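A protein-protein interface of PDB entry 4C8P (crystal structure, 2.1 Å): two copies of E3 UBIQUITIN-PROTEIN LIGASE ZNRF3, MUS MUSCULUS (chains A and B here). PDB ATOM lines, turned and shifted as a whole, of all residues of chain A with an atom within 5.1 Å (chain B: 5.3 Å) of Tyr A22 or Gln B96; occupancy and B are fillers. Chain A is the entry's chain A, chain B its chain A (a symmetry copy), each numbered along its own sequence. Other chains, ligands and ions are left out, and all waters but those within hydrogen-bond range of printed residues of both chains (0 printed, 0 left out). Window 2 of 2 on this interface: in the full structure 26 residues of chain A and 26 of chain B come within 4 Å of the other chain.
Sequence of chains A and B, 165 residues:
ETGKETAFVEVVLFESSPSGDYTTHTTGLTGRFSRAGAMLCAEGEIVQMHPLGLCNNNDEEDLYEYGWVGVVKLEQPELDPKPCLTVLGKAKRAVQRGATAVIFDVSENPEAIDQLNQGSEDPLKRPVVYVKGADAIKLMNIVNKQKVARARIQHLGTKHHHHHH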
ATOM      1  N   PHE A  14      21.014  12.571  -9.198  1.00  0.00           N
ATOM      2  CA  PHE A  14      20.768  11.464  -8.316  1.00  0.00           C
ATOM      3  C   PHE A  14      19.508  11.589  -7.438  1.00  0.00           C
ATOM      4  O   PHE A  14      19.111  12.673  -7.026  1.00  0.00           O
ATOM      5  CB  PHE A  14      21.985  11.222  -7.421  1.00  0.00           C
ATOM      6  CG  PHE A  14      22.503  12.441  -6.803  1.00  0.00           C
ATOM      7  CD1 PHE A  14      23.429  13.223  -7.470  1.00  0.00           C
ATOM      8  CD2 PHE A  14      22.055  12.844  -5.570  1.00  0.00           C
ATOM      9  CE1 PHE A  14      23.916  14.392  -6.903  1.00  0.00           C
ATOM     10  CE2 PHE A  14      22.520  14.028  -5.000  1.00  0.00           C
ATOM     11  CZ  PHE A  14      23.462  14.793  -5.668  1.00  0.00           C
ATOM     12  N   GLU A  15      18.933  10.429  -7.133  1.00  0.00           N
ATOM     13  CA  GLU A  15      17.754  10.311  -6.312  1.00  0.00           C
ATOM     14  C   GLU A  15      17.874   9.023  -5.494  1.00  0.00           C
ATOM     15  O   GLU A  15      18.329   8.014  -6.001  1.00  0.00           O
ATOM     16  CB  GLU A  15      16.527  10.275  -7.208  1.00  0.00           C
ATOM     17  CG  GLU A  15      15.371  11.101  -6.657  1.00  0.00           C
ATOM     18  CD  GLU A  15      14.043  10.768  -7.323  1.00  0.00           C
ATOM     19  OE1 GLU A  15      14.056  10.175  -8.428  1.00  0.00           O
ATOM     20  OE2 GLU A  15      12.984  11.089  -6.738  1.00  0.00           O
ATOM     21  N   SER A  16      17.505   9.061  -4.221  1.00  0.00           N
ATOM     22  CA  SER A  16      17.567   7.865  -3.377  1.00  0.00           C
ATOM     23  C   SER A  16      16.205   7.269  -3.268  1.00  0.00           C
ATOM     24  O   SER A  16      15.226   7.917  -3.583  1.00  0.00           O
ATOM     25  CB  SER A  16      18.052   8.194  -1.980  1.00  0.00           C
ATOM     26  OG  SER A  16      17.364   9.336  -1.573  1.00  0.00           O
ATOM     27  N   GLY A  20      17.256   3.399   0.464  1.00  0.00           N
ATOM     28  CA  GLY A  20      18.551   4.057   0.692  1.00  0.00           C
ATOM     29  C   GLY A  20      19.612   3.822  -0.395  1.00  0.00           C
ATOM     30  O   GLY A  20      20.767   4.079  -0.162  1.00  0.00           O
ATOM     31  N   ASP A  21      19.204   3.308  -1.556  1.00  0.00           N
ATOM     32  CA  ASP A  21      20.068   3.087  -2.730  1.00  0.00           C
ATOM     33  C   ASP A  21      19.828   4.244  -3.664  1.00  0.00           C
ATOM     34  O   ASP A  21      18.687   4.706  -3.826  1.00  0.00           O
ATOM     35  CB  ASP A  21      19.718   1.796  -3.513  1.00  0.00           C
ATOM     36  CG  ASP A  21      20.073   0.495  -2.758  1.00  0.00           C
ATOM     37  OD1 ASP A  21      20.826   0.525  -1.751  1.00  0.00           O
ATOM     38  OD2 ASP A  21      19.604  -0.598  -3.186  1.00  0.00           O
ATOM     39  N   TYR A  22      20.893   4.713  -4.292  1.00  0.00           N
ATOM     40  CA  TYR A  22      20.747   5.825  -5.211  1.00  0.00           C
ATOM     41  C   TYR A  22      20.473   5.387  -6.642  1.00  0.00           C
ATOM     42  O   TYR A  22      20.997   4.375  -7.130  1.00  0.00           O
ATOM     43  CB  TYR A  22      21.965   6.725  -5.176  1.00  0.00           C
ATOM     44  CG  TYR A  22      21.947   7.659  -4.023  1.00  0.00           C
ATOM     45  CD1 TYR A  22      22.497   7.300  -2.830  1.00  0.00           C
ATOM     46  CD2 TYR A  22      21.359   8.898  -4.132  1.00  0.00           C
ATOM     47  CE1 TYR A  22      22.504   8.166  -1.775  1.00  0.00           C
ATOM     48  CE2 TYR A  22      21.344   9.773  -3.075  1.00  0.00           C
ATOM     49  CZ  TYR A  22      21.924   9.404  -1.907  1.00  0.00           C
ATOM     50  OH  TYR A  22      21.894  10.251  -0.829  1.00  0.00           O
ATOM     51  N   THR A  23      19.606   6.164  -7.286  1.00  0.00           N
ATOM     52  CA  THR A  23      19.419   6.134  -8.712  1.00  0.00           C
ATOM     53  C   THR A  23      20.168   7.370  -9.241  1.00  0.00           C
ATOM     54  O   THR A  23      20.010   8.495  -8.703  1.00  0.00           O
ATOM     55  CB  THR A  23      17.916   6.189  -9.067  1.00  0.00           C
ATOM     56  OG1 THR A  23      17.264   5.022  -8.548  1.00  0.00           O
ATOM     57  CG2 THR A  23      17.712   6.269 -10.568  1.00  0.00           C
ATOM     58  N   THR A  24      21.014   7.145 -10.244  1.00  0.00           N
ATOM     59  CA  THR A  24      21.815   8.220 -10.848  1.00  0.00           C
ATOM     60  C   THR A  24      21.513   8.368 -12.323  1.00  0.00           C
ATOM     61  O   THR A  24      21.003   7.428 -12.965  1.00  0.00           O
ATOM     62  CB  THR A  24      23.346   8.014 -10.690  1.00  0.00           C
ATOM     63  OG1 THR A  24      23.761   6.816 -11.355  1.00  0.00           O
ATOM     64  CG2 THR A  24      23.742   7.961  -9.247  1.00  0.00           C
ATOM     65  N   LEU B  63      21.652   6.643   5.882  1.00  0.00           N
ATOM     66  CA  LEU B  63      21.733   7.307   4.574  1.00  0.00           C
ATOM     67  C   LEU B  63      22.727   8.482   4.559  1.00  0.00           C
ATOM     68  O   LEU B  63      22.758   9.292   5.493  1.00  0.00           O
ATOM     69  CB  LEU B  63      20.360   7.804   4.101  1.00  0.00           C
ATOM     70  CG  LEU B  63      20.391   8.452   2.689  1.00  0.00           C
ATOM     71  CD1 LEU B  63      20.452   7.407   1.575  1.00  0.00           C
ATOM     72  CD2 LEU B  63      19.219   9.414   2.466  1.00  0.00           C
ATOM     73  N   TYR B  64      23.513   8.550   3.478  1.00  0.00           N
ATOM     74  CA  TYR B  64      24.543   9.576   3.230  1.00  0.00           C
ATOM     75  C   TYR B  64      24.293  10.237   1.870  1.00  0.00           C
ATOM     76  O   TYR B  64      23.782   9.607   0.929  1.00  0.00           O
ATOM     77  CB  TYR B  64      25.962   8.957   3.215  1.00  0.00           C
ATOM     78  CG  TYR B  64      26.316   8.271   4.502  1.00  0.00           C
ATOM     79  CD1 TYR B  64      26.670   9.017   5.633  1.00  0.00           C
ATOM     80  CD2 TYR B  64      26.256   6.877   4.613  1.00  0.00           C
ATOM     81  CE1 TYR B  64      26.977   8.397   6.836  1.00  0.00           C
ATOM     82  CE2 TYR B  64      26.549   6.240   5.812  1.00  0.00           C
ATOM     83  CZ  TYR B  64      26.905   7.016   6.922  1.00  0.00           C
ATOM     84  OH  TYR B  64      27.199   6.403   8.121  1.00  0.00           O
ATOM     85  N   GLU B  65      24.665  11.505   1.768  1.00  0.00           N
ATOM     86  CA  GLU B  65      24.447  12.260   0.548  1.00  0.00           C
ATOM     87  C   GLU B  65      25.384  11.706  -0.558  1.00  0.00           C
ATOM     88  O   GLU B  65      26.554  11.339  -0.302  1.00  0.00           O
ATOM     89  CB  GLU B  65      24.577  13.787   0.809  1.00  0.00           C
ATOM     90  CG  GLU B  65      24.580  14.718  -0.430  1.00  0.00           C
ATOM     91  CD  GLU B  65      23.278  14.797  -1.260  1.00  0.00           C
ATOM     92  OE1 GLU B  65      22.475  13.826  -1.363  1.00  0.00           O
ATOM     93  OE2 GLU B  65      23.072  15.869  -1.869  1.00  0.00           O
ATOM     94  N   TYR B  66      24.826  11.606  -1.770  1.00  0.00           N
ATOM     95  CA  TYR B  66      25.502  11.007  -2.907  1.00  0.00           C
ATOM     96  C   TYR B  66      26.949  11.544  -2.990  1.00  0.00           C
ATOM     97  O   TYR B  66      27.170  12.720  -2.781  1.00  0.00           O
ATOM     98  CB  TYR B  66      24.711  11.236  -4.220  1.00  0.00           C
ATOM     99  CG  TYR B  66      25.391  10.552  -5.398  1.00  0.00           C
ATOM    100  CD1 TYR B  66      25.251   9.193  -5.632  1.00  0.00           C
ATOM    101  CD2 TYR B  66      26.230  11.264  -6.230  1.00  0.00           C
ATOM    102  CE1 TYR B  66      25.923   8.569  -6.697  1.00  0.00           C
ATOM    103  CE2 TYR B  66      26.924  10.659  -7.273  1.00  0.00           C
ATOM    104  CZ  TYR B  66      26.775   9.313  -7.505  1.00  0.00           C
ATOM    105  OH  TYR B  66      27.478   8.772  -8.570  1.00  0.00           O
ATOM    106  N   ALA B  91      31.800  -3.406  -1.262  1.00  0.00           N
ATOM    107  CA  ALA B  91      32.102  -2.273  -2.109  1.00  0.00           C
ATOM    108  C   ALA B  91      31.003  -1.910  -3.142  1.00  0.00           C
ATOM    109  O   ALA B  91      30.878  -0.745  -3.444  1.00  0.00           O
ATOM    110  CB  ALA B  91      33.441  -2.502  -2.836  1.00  0.00           C
ATOM    111  N   LYS B  92      30.270  -2.872  -3.721  1.00  0.00           N
ATOM    112  CA  LYS B  92      29.173  -2.552  -4.628  1.00  0.00           C
ATOM    113  C   LYS B  92      28.026  -2.069  -3.785  1.00  0.00           C
ATOM    114  O   LYS B  92      27.307  -1.178  -4.159  1.00  0.00           O
ATOM    115  CB  LYS B  92      28.717  -3.757  -5.440  1.00  0.00           C
ATOM    116  CG  LYS B  92      29.839  -4.602  -6.031  1.00  0.00           C
ATOM    117  CD  LYS B  92      29.279  -5.745  -6.889  1.00  0.00           C
ATOM    118  CE  LYS B  92      30.298  -6.318  -7.873  1.00  0.00           C
ATOM    119  NZ  LYS B  92      30.299  -5.633  -9.219  1.00  0.00           N
ATOM    120  N   ARG B  93      27.902  -2.616  -2.602  1.00  0.00           N
ATOM    121  CA  ARG B  93      26.870  -2.185  -1.710  1.00  0.00           C
ATOM    122  C   ARG B  93      27.083  -0.698  -1.353  1.00  0.00           C
ATOM    123  O   ARG B  93      26.138   0.096  -1.324  1.00  0.00           O
ATOM    124  CB  ARG B  93      26.918  -3.111  -0.504  1.00  0.00           C
ATOM    125  CG  ARG B  93      25.665  -3.227   0.291  1.00  0.00           C
ATOM    126  CD  ARG B  93      24.441  -3.668  -0.519  1.00  0.00           C
ATOM    127  NE  ARG B  93      23.367  -3.047   0.260  1.00  0.00           N
ATOM    128  CZ  ARG B  93      22.504  -2.131  -0.144  1.00  0.00           C
ATOM    129  NH1 ARG B  93      22.415  -1.736  -1.405  1.00  0.00           N
ATOM    130  NH2 ARG B  93      21.668  -1.629   0.760  1.00  0.00           N
ATOM    131  N   ALA B  94      28.355  -0.321  -1.195  1.00  0.00           N
ATOM    132  CA  ALA B  94      28.719   1.035  -0.818  1.00  0.00           C
ATOM    133  C   ALA B  94      28.373   1.969  -1.947  1.00  0.00           C
ATOM    134  O   ALA B  94      27.737   3.017  -1.742  1.00  0.00           O
ATOM    135  CB  ALA B  94      30.214   1.113  -0.510  1.00  0.00           C
ATOM    136  N   VAL B  95      28.744   1.561  -3.155  1.00  0.00           N
ATOM    137  CA  VAL B  95      28.413   2.333  -4.318  1.00  0.00           C
ATOM    138  C   VAL B  95      26.899   2.423  -4.597  1.00  0.00           C
ATOM    139  O   VAL B  95      26.391   3.460  -4.996  1.00  0.00           O
ATOM    140  CB  VAL B  95      29.134   1.730  -5.542  1.00  0.00           C
ATOM    141  CG1 VAL B  95      28.652   2.375  -6.790  1.00  0.00           C
ATOM    142  CG2 VAL B  95      30.656   1.888  -5.409  1.00  0.00           C
ATOM    143  N   GLN B  96      26.165   1.337  -4.440  1.00  0.00           N
ATOM    144  CA  GLN B  96      24.702   1.411  -4.526  1.00  0.00           C
ATOM    145  C   GLN B  96      24.104   2.458  -3.578  1.00  0.00           C
ATOM    146  O   GLN B  96      23.096   3.048  -3.865  1.00  0.00           O
ATOM    147  CB  GLN B  96      24.119   0.059  -4.181  1.00  0.00           C
ATOM    148  CG  GLN B  96      24.441  -0.995  -5.227  1.00  0.00           C
ATOM    149  CD  GLN B  96      23.815  -2.328  -4.922  1.00  0.00           C
ATOM    150  OE1 GLN B  96      23.361  -2.600  -3.785  1.00  0.00           O
ATOM    151  NE2 GLN B  96      23.752  -3.172  -5.922  1.00  0.00           N
ATOM    152  N   ARG B  97      24.769   2.683  -2.451  1.00  0.00           N
ATOM    153  CA  ARG B  97      24.366   3.666  -1.448  1.00  0.00           C
ATOM    154  C   ARG B  97      25.096   4.996  -1.619  1.00  0.00           C
ATOM    155  O   ARG B  97      25.248   5.726  -0.653  1.00  0.00           O
ATOM    156  CB  ARG B  97      24.616   3.083  -0.051  1.00  0.00           C
ATOM    157  CG  ARG B  97      23.850   1.781   0.145  1.00  0.00           C
ATOM    158  CD  ARG B  97      24.374   0.961   1.289  1.00  0.00           C
ATOM    159  NE  ARG B  97      24.161   1.638   2.545  1.00  0.00           N
ATOM    160  CZ  ARG B  97      24.697   1.263   3.704  1.00  0.00           C
ATOM    161  NH1 ARG B  97      25.477   0.187   3.776  1.00  0.00           N
ATOM    162  NH2 ARG B  97      24.464   1.989   4.794  1.00  0.00           N
ATOM    163  N   GLY B  98      25.519   5.328  -2.844  1.00  0.00           N
ATOM    164  CA  GLY B  98      26.053   6.657  -3.134  1.00  0.00           C
ATOM    165  C   GLY B  98      27.575   6.919  -3.005  1.00  0.00           C
ATOM    166  O   GLY B  98      28.032   8.066  -3.131  1.00  0.00           O
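No position is printed for both chains.
The side-chain carboxylate (OD1) of Asp A21 lies within salt-bridge range of the guanidinium group (NH1) of Arg B93.
OH of Tyr A22 lies within hydrogen-bond range of O of Tyr B64 (2.7 Å).
The backbone NH (N) of Tyr B66 sits at hydrogen-bond distance from the side-chain hydroxyl (OH) of Tyr A22 (3.4 Å).
The backbone NH of Tyr A22 lies within hydrogen-bond range of the backbone carbonyl oxygen of Gln B96, at 2.8 Å.
Among the printed residues, merely in contact across the chains: Phe A14 with Glu B65 (3.6 Å), Phe A14 with Tyr B66 (3.4 Å), Gly A20 with Leu B63 (3.8 Å), Gly A20 with Arg B97 (3.8 Å), Asp A21 with Gln B96 (3.2 Å), Asp A21 with Arg B97 (3.8 Å), Tyr A22 with Leu B63 (3.99 Å), Tyr A22 with Glu B65 (3.5 Å), Tyr A22 with Arg B97 (3.7 Å), Tyr A22 with Gly B98 (3.6 Å) and Thr A24 with Tyr B66 (3.4 Å).
Of the 12 printed residues of chain B, 8 touch a printed residue of chain A.
Hydrophobic or aromatic side chains of chain A within 4 Å of the printed part of chain B: Phe A14 and Tyr A22.
Among the printed residues, Asp or Glu carboxylates within 4 Å of a Lys or Arg side-chain nitrogen of the other chain: Asp A21 with Arg B93.
Of the printed residues of chain B, Phe A14 touches Glu B65 and Tyr B66.
Of the printed residues of chain B, Tyr A22 touches Leu B63, Tyr B64, Glu B65, Tyr B66, Gln B96, Arg B97 and Gly B98.
Of the printed residues of chain B, Thr A24 touches Tyr B66.
Of the printed residues of chain A, Arg B93 touches Asp A21.
Of chain A, only Asp A21 (3.2 Å) and Tyr A22 (2.8 Å) come within 4 Å of Gln B96.
Of the printed residues of chain A, Arg B97 touches Gly A20, Asp A21 and Tyr A22.
The side-chain amide oxygen (OE1) of Gln B96 is in hydrogen-bond range of the guanidinium group (NH1) of Arg B93 (2.7 Å).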
